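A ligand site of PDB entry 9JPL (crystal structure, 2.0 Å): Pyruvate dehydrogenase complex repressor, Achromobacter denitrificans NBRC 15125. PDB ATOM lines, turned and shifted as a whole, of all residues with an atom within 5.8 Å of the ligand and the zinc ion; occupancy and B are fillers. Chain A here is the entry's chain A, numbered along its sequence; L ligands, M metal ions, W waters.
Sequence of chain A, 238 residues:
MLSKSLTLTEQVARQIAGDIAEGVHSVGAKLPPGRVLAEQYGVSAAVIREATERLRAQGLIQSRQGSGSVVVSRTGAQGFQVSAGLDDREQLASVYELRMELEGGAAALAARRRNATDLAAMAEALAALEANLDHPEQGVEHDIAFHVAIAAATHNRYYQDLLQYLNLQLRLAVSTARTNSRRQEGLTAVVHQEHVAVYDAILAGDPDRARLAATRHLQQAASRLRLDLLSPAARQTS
O of Ala 177 lies close to O5 of the ligand.
Val 174 touches the ligand.
Arg 178 touches the ligand.
CG2 of Val 191 touches O5 of the ligand, 3.6 Å away.
CB of Ala 221 touches O4 of the ligand, 3.6 Å away.
Hydrophobic or aromatic side chains that line the ligand: Tyr 96, His 147, Val 174, Ala 177, Val 191, His 195, His 217 and Ala 221.
Of the 19 residues printed, 13 come within 4 Å of the ligand.
The nearest printed residue that does not touch the ligand is Leu 218 (4.5 Å).
Water W1 lies within hydrogen-bond range of O4 of the ligand (2.8 Å), O of Ala 221 (2.9 Å) and NE of Arg 224 (3.5 Å).
OG of Ser 181 is in hydrogen-bond range of O5 of the ligand (2.5 Å).
NH1 of Arg 99 is in salt-bridge range of O1 of the ligand, 2.7 Å away.
The side-chain hydroxyl (OH) of Tyr 96 sits at hydrogen-bond distance from an oxygen (O1) of the ligand, 2.8 Å away.
O4 of the ligand lies within salt-bridge range of NH2 of Arg 224 (2.9 Å).
Four residues have an atom within 4 Å of the zinc ion: Asp 143, His 147, His 195 and His 217.
The zinc ion is bound by O2 of the ligand, NE2 of His 147, NE2 of His 195, O3 of the ligand, NE2 of His 217 and OD1 of Asp 143.
A ring nitrogen (ND1) of His 147 sits at hydrogen-bond distance from the side-chain carboxylate of Glu 103, at 3.2 Å.
The side-chain carboxylate (OE1) of Glu 194 sits at hydrogen-bond distance from a ring nitrogen (ND1) of His 217 (2.8 Å).
The side-chain carboxylate (OD2) of Asp 143 lies within salt-bridge range of the guanidinium group (NH1) of Arg 178 (2.8 Å).
OG of Ser 181 is in hydrogen-bond range of O of Ala 177 (3.3 Å).
The side-chain carboxylate (OE2) of Glu 103 lies within salt-bridge range of the guanidinium group (NE) of Arg 99 (2.6 Å).
OH of Tyr 96 is in hydrogen-bond range of O of Ala 173 (3.4 Å).
The guanidinium group of Arg 224 lies within salt-bridge range of the side-chain carboxylate of Glu 194, at 2.8 Å.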
ATOM      1  N   TYR A  96     -21.444 -34.983 -10.819  1.00  0.00           N
ATOM      2  CA  TYR A  96     -20.312 -35.143  -9.919  1.00  0.00           C
ATOM      3  C   TYR A  96     -19.592 -36.474 -10.149  1.00  0.00           C
ATOM      4  O   TYR A  96     -18.355 -36.517 -10.089  1.00  0.00           O
ATOM      5  CB  TYR A  96     -20.771 -34.979  -8.460  1.00  0.00           C
ATOM      6  CG  TYR A  96     -20.739 -33.502  -8.071  1.00  0.00           C
ATOM      7  CD1 TYR A  96     -19.524 -32.829  -7.909  1.00  0.00           C
ATOM      8  CD2 TYR A  96     -21.915 -32.775  -7.900  1.00  0.00           C
ATOM      9  CE1 TYR A  96     -19.493 -31.479  -7.586  1.00  0.00           C
ATOM     10  CE2 TYR A  96     -21.895 -31.416  -7.576  1.00  0.00           C
ATOM     11  CZ  TYR A  96     -20.679 -30.772  -7.424  1.00  0.00           C
ATOM     12  OH  TYR A  96     -20.648 -29.432  -7.102  1.00  0.00           O
ATOM     13  N   ARG A  99     -17.436 -35.820 -13.240  1.00  0.00           N
ATOM     14  CA  ARG A  99     -16.353 -34.902 -12.897  1.00  0.00           C
ATOM     15  C   ARG A  99     -15.254 -35.619 -12.126  1.00  0.00           C
ATOM     16  O   ARG A  99     -14.074 -35.332 -12.307  1.00  0.00           O
ATOM     17  CB  ARG A  99     -16.908 -33.730 -12.081  1.00  0.00           C
ATOM     18  CG  ARG A  99     -17.672 -32.690 -12.918  1.00  0.00           C
ATOM     19  CD  ARG A  99     -18.170 -31.527 -12.060  1.00  0.00           C
ATOM     20  NE  ARG A  99     -17.046 -30.669 -11.675  1.00  0.00           N
ATOM     21  CZ  ARG A  99     -17.099 -29.745 -10.719  1.00  0.00           C
ATOM     22  NH1 ARG A  99     -18.241 -29.543 -10.049  1.00  0.00           N
ATOM     23  NH2 ARG A  99     -16.013 -29.025 -10.445  1.00  0.00           N
ATOM     24  N   GLU A 103     -12.010 -34.975 -13.920  1.00  0.00           N
ATOM     25  CA  GLU A 103     -11.172 -33.975 -13.275  1.00  0.00           C
ATOM     26  C   GLU A 103     -10.085 -34.607 -12.407  1.00  0.00           C
ATOM     27  O   GLU A 103      -9.019 -34.012 -12.257  1.00  0.00           O
ATOM     28  CB  GLU A 103     -12.024 -33.002 -12.433  1.00  0.00           C
ATOM     29  CG  GLU A 103     -12.868 -32.085 -13.315  1.00  0.00           C
ATOM     30  CD  GLU A 103     -13.754 -31.070 -12.547  1.00  0.00           C
ATOM     31  OE1 GLU A 103     -13.381 -30.621 -11.441  1.00  0.00           O
ATOM     32  OE2 GLU A 103     -14.833 -30.745 -13.074  1.00  0.00           O
ATOM     33  N   ASP A 143     -14.845 -20.329  -9.913  1.00  0.00           N
ATOM     34  CA  ASP A 143     -14.755 -21.745  -9.568  1.00  0.00           C
ATOM     35  C   ASP A 143     -14.637 -22.600 -10.823  1.00  0.00           C
ATOM     36  O   ASP A 143     -13.713 -23.413 -10.951  1.00  0.00           O
ATOM     37  CB  ASP A 143     -16.009 -22.118  -8.742  1.00  0.00           C
ATOM     38  CG  ASP A 143     -15.869 -23.432  -7.935  1.00  0.00           C
ATOM     39  OD1 ASP A 143     -15.260 -24.396  -8.427  1.00  0.00           O
ATOM     40  OD2 ASP A 143     -16.440 -23.510  -6.803  1.00  0.00           O
ATOM     41  N   PHE A 146     -11.268 -22.071 -12.570  1.00  0.00           N
ATOM     42  CA  PHE A 146     -10.187 -22.813 -11.929  1.00  0.00           C
ATOM     43  C   PHE A 146     -10.145 -24.260 -12.428  1.00  0.00           C
ATOM     44  O   PHE A 146      -9.087 -24.762 -12.826  1.00  0.00           O
ATOM     45  CB  PHE A 146     -10.356 -22.756 -10.405  1.00  0.00           C
ATOM     46  CG  PHE A 146      -9.361 -23.609  -9.644  1.00  0.00           C
ATOM     47  CD1 PHE A 146      -8.037 -23.180  -9.467  1.00  0.00           C
ATOM     48  CD2 PHE A 146      -9.740 -24.850  -9.103  1.00  0.00           C
ATOM     49  CE1 PHE A 146      -7.114 -23.974  -8.754  1.00  0.00           C
ATOM     50  CE2 PHE A 146      -8.818 -25.634  -8.389  1.00  0.00           C
ATOM     51  CZ  PHE A 146      -7.507 -25.196  -8.230  1.00  0.00           C
ATOM     52  N   HIS A 147     -11.289 -24.947 -12.450  1.00  0.00           N
ATOM     53  CA  HIS A 147     -11.306 -26.339 -12.908  1.00  0.00           C
ATOM     54  C   HIS A 147     -10.988 -26.429 -14.395  1.00  0.00           C
ATOM     55  O   HIS A 147     -10.271 -27.340 -14.819  1.00  0.00           O
ATOM     56  CB  HIS A 147     -12.656 -26.974 -12.584  1.00  0.00           C
ATOM     57  CG  HIS A 147     -12.924 -27.071 -11.112  1.00  0.00           C
ATOM     58  ND1 HIS A 147     -12.166 -27.870 -10.285  1.00  0.00           N
ATOM     59  CD2 HIS A 147     -13.794 -26.417 -10.322  1.00  0.00           C
ATOM     60  CE1 HIS A 147     -12.583 -27.714  -9.034  1.00  0.00           C
ATOM     61  NE2 HIS A 147     -13.571 -26.847  -9.036  1.00  0.00           N
ATOM     62  N   ALA A 173     -23.960 -27.649 -11.380  1.00  0.00           N
ATOM     63  CA  ALA A 173     -23.405 -28.267 -10.192  1.00  0.00           C
ATOM     64  C   ALA A 173     -22.754 -27.221  -9.284  1.00  0.00           C
ATOM     65  O   ALA A 173     -23.017 -27.194  -8.071  1.00  0.00           O
ATOM     66  CB  ALA A 173     -22.380 -29.333 -10.577  1.00  0.00           C
ATOM     67  N   VAL A 174     -21.900 -26.372  -9.861  1.00  0.00           N
ATOM     68  CA  VAL A 174     -21.136 -25.414  -9.054  1.00  0.00           C
ATOM     69  C   VAL A 174     -22.056 -24.364  -8.432  1.00  0.00           C
ATOM     70  O   VAL A 174     -21.891 -23.990  -7.258  1.00  0.00           O
ATOM     71  CB  VAL A 174     -20.023 -24.778  -9.899  1.00  0.00           C
ATOM     72  CG1 VAL A 174     -19.387 -23.584  -9.166  1.00  0.00           C
ATOM     73  CG2 VAL A 174     -18.920 -25.829 -10.296  1.00  0.00           C
ATOM     74  N   ALA A 177     -23.923 -26.055  -5.556  1.00  0.00           N
ATOM     75  CA  ALA A 177     -23.016 -26.327  -4.446  1.00  0.00           C
ATOM     76  C   ALA A 177     -22.661 -25.071  -3.668  1.00  0.00           C
ATOM     77  O   ALA A 177     -22.730 -25.044  -2.444  1.00  0.00           O
ATOM     78  CB  ALA A 177     -21.741 -27.011  -4.963  1.00  0.00           C
ATOM     79  N   ARG A 178     -22.266 -24.001  -4.381  1.00  0.00           N
ATOM     80  CA  ARG A 178     -21.795 -22.815  -3.674  1.00  0.00           C
ATOM     81  C   ARG A 178     -22.934 -22.135  -2.914  1.00  0.00           C
ATOM     82  O   ARG A 178     -22.751 -21.678  -1.789  1.00  0.00           O
ATOM     83  CB  ARG A 178     -21.117 -21.856  -4.656  1.00  0.00           C
ATOM     84  CG  ARG A 178     -19.822 -22.454  -5.284  1.00  0.00           C
ATOM     85  CD  ARG A 178     -19.164 -21.466  -6.251  1.00  0.00           C
ATOM     86  NE  ARG A 178     -18.622 -20.339  -5.496  1.00  0.00           N
ATOM     87  CZ  ARG A 178     -17.443 -20.340  -4.900  1.00  0.00           C
ATOM     88  NH1 ARG A 178     -16.650 -21.403  -4.998  1.00  0.00           N
ATOM     89  NH2 ARG A 178     -17.058 -19.279  -4.216  1.00  0.00           N
ATOM     90  N   SER A 181     -23.357 -24.136   0.214  1.00  0.00           N
ATOM     91  CA  SER A 181     -22.292 -23.993   1.206  1.00  0.00           C
ATOM     92  C   SER A 181     -22.343 -22.658   1.945  1.00  0.00           C
ATOM     93  O   SER A 181     -21.889 -22.568   3.096  1.00  0.00           O
ATOM     94  CB  SER A 181     -20.917 -24.173   0.552  1.00  0.00           C
ATOM     95  OG  SER A 181     -20.722 -25.528   0.176  1.00  0.00           O
ATOM     96  N   VAL A 191     -14.164 -24.968   1.747  1.00  0.00           N
ATOM     97  CA  VAL A 191     -14.181 -25.352   0.338  1.00  0.00           C
ATOM     98  C   VAL A 191     -13.011 -24.708  -0.394  1.00  0.00           C
ATOM     99  O   VAL A 191     -12.387 -25.332  -1.259  1.00  0.00           O
ATOM    100  CB  VAL A 191     -15.530 -24.997  -0.300  1.00  0.00           C
ATOM    101  CG1 VAL A 191     -15.478 -25.170  -1.842  1.00  0.00           C
ATOM    102  CG2 VAL A 191     -16.591 -25.889   0.305  1.00  0.00           C
ATOM    103  N   GLU A 194     -10.029 -26.759  -0.286  1.00  0.00           N
ATOM    104  CA  GLU A 194     -10.093 -27.870  -1.222  1.00  0.00           C
ATOM    105  C   GLU A 194      -9.524 -27.490  -2.585  1.00  0.00           C
ATOM    106  O   GLU A 194      -8.835 -28.292  -3.224  1.00  0.00           O
ATOM    107  CB  GLU A 194     -11.539 -28.387  -1.375  1.00  0.00           C
ATOM    108  CG  GLU A 194     -12.136 -28.955  -0.076  1.00  0.00           C
ATOM    109  CD  GLU A 194     -13.630 -29.266  -0.183  1.00  0.00           C
ATOM    110  OE1 GLU A 194     -14.217 -29.246  -1.300  1.00  0.00           O
ATOM    111  OE2 GLU A 194     -14.228 -29.543   0.884  1.00  0.00           O
ATOM    112  N   HIS A 195      -9.822 -26.271  -3.059  1.00  0.00           N
ATOM    113  CA  HIS A 195      -9.234 -25.795  -4.319  1.00  0.00           C
ATOM    114  C   HIS A 195      -7.729 -25.586  -4.177  1.00  0.00           C
ATOM    115  O   HIS A 195      -6.968 -25.919  -5.091  1.00  0.00           O
ATOM    116  CB  HIS A 195      -9.890 -24.487  -4.777  1.00  0.00           C
ATOM    117  CG  HIS A 195     -11.288 -24.643  -5.277  1.00  0.00           C
ATOM    118  ND1 HIS A 195     -12.285 -23.709  -5.033  1.00  0.00           N
ATOM    119  CD2 HIS A 195     -11.874 -25.635  -5.989  1.00  0.00           C
ATOM    120  CE1 HIS A 195     -13.410 -24.128  -5.582  1.00  0.00           C
ATOM    121  NE2 HIS A 195     -13.189 -25.290  -6.177  1.00  0.00           N
ATOM    122  N   HIS A 217     -12.211 -33.157  -3.461  1.00  0.00           N
ATOM    123  CA  HIS A 217     -13.023 -31.945  -3.566  1.00  0.00           C
ATOM    124  C   HIS A 217     -14.421 -32.271  -4.072  1.00  0.00           C
ATOM    125  O   HIS A 217     -15.428 -31.784  -3.531  1.00  0.00           O
ATOM    126  CB  HIS A 217     -12.299 -30.946  -4.492  1.00  0.00           C
ATOM    127  CG  HIS A 217     -13.135 -29.770  -4.919  1.00  0.00           C
ATOM    128  ND1 HIS A 217     -13.801 -28.938  -4.039  1.00  0.00           N
ATOM    129  CD2 HIS A 217     -13.337 -29.230  -6.152  1.00  0.00           C
ATOM    130  CE1 HIS A 217     -14.404 -27.968  -4.701  1.00  0.00           C
ATOM    131  NE2 HIS A 217     -14.134 -28.121  -5.991  1.00  0.00           N
ATOM    132  N   LEU A 218     -14.515 -33.119  -5.104  1.00  0.00           N
ATOM    133  CA  LEU A 218     -15.807 -33.435  -5.706  1.00  0.00           C
ATOM    134  C   LEU A 218     -16.620 -34.377  -4.816  1.00  0.00           C
ATOM    135  O   LEU A 218     -17.853 -34.270  -4.752  1.00  0.00           O
ATOM    136  CB  LEU A 218     -15.585 -34.016  -7.097  1.00  0.00           C
ATOM    137  CG  LEU A 218     -14.828 -33.046  -8.019  1.00  0.00           C
ATOM    138  CD1 LEU A 218     -14.344 -33.750  -9.261  1.00  0.00           C
ATOM    139  CD2 LEU A 218     -15.709 -31.815  -8.386  1.00  0.00           C
ATOM    140  N   GLN A 220     -16.496 -34.361  -1.485  1.00  0.00           N
ATOM    141  CA  GLN A 220     -17.006 -33.562  -0.377  1.00  0.00           C
ATOM    142  C   GLN A 220     -18.151 -32.662  -0.831  1.00  0.00           C
ATOM    143  O   GLN A 220     -19.109 -32.453  -0.075  1.00  0.00           O
ATOM    144  CB  GLN A 220     -15.868 -32.744   0.227  1.00  0.00           C
ATOM    145  CG  GLN A 220     -14.804 -33.618   0.896  1.00  0.00           C
ATOM    146  CD  GLN A 220     -15.400 -34.478   2.001  1.00  0.00           C
ATOM    147  OE1 GLN A 220     -15.371 -35.706   1.937  1.00  0.00           O
ATOM    148  NE2 GLN A 220     -15.953 -33.837   3.018  1.00  0.00           N
ATOM    149  N   ALA A 221     -18.058 -32.107  -2.046  1.00  0.00           N
ATOM    150  CA  ALA A 221     -19.159 -31.301  -2.581  1.00  0.00           C
ATOM    151  C   ALA A 221     -20.421 -32.139  -2.723  1.00  0.00           C
ATOM    152  O   ALA A 221     -21.521 -31.698  -2.362  1.00  0.00           O
ATOM    153  CB  ALA A 221     -18.753 -30.692  -3.920  1.00  0.00           C
ATOM    154  N   ARG A 224     -21.714 -32.704   0.772  1.00  0.00           N
ATOM    155  CA  ARG A 224     -22.382 -31.524   1.301  1.00  0.00           C
ATOM    156  C   ARG A 224     -23.804 -31.389   0.767  1.00  0.00           C
ATOM    157  O   ARG A 224     -24.695 -30.913   1.472  1.00  0.00           O
ATOM    158  CB  ARG A 224     -21.591 -30.259   0.963  1.00  0.00           C
ATOM    159  CG  ARG A 224     -20.356 -30.040   1.833  1.00  0.00           C
ATOM    160  CD  ARG A 224     -19.700 -28.702   1.497  1.00  0.00           C
ATOM    161  NE  ARG A 224     -18.950 -28.709   0.234  1.00  0.00           N
ATOM    162  CZ  ARG A 224     -17.688 -29.111   0.104  1.00  0.00           C
ATOM    163  NH1 ARG A 224     -17.022 -29.575   1.151  1.00  0.00           N
ATOM    164  NH2 ARG A 224     -17.091 -29.060  -1.074  1.00  0.00           N
HETATM  165  C1  LIG L   1     -17.326 -27.384  -7.375  1.00  0.00           C
HETATM  166  O1  LIG L   1     -18.238 -28.184  -7.668  1.00  0.00           O
HETATM  167  C2  LIG L   1     -17.501 -26.376  -6.237  1.00  0.00           C
HETATM  168  O2  LIG L   1     -16.263 -27.369  -8.066  1.00  0.00           O
HETATM  169  C3  LIG L   1     -18.109 -26.954  -4.957  1.00  0.00           C
HETATM  170  O3  LIG L   1     -16.238 -25.817  -5.934  1.00  0.00           O
HETATM  171  C4  LIG L   1     -18.435 -25.732  -4.071  1.00  0.00           C
HETATM  172  O4  LIG L   1     -19.096 -27.394  -2.443  1.00  0.00           O
HETATM  173  C5  LIG L   1     -19.002 -26.181  -2.722  1.00  0.00           C
HETATM  174  O5  LIG L   1     -19.390 -25.322  -1.872  1.00  0.00           O
HETATM  175 ZN    ZN M   1     -14.644 -26.382  -7.283  1.00  0.00          ZN
HETATM  176  O   HOH W   1     -21.539 -28.793  -2.101  1.00  0.00           O
HETATM  177  O   HOH W   2     -18.375 -22.857  -1.881  1.00  0.00           O
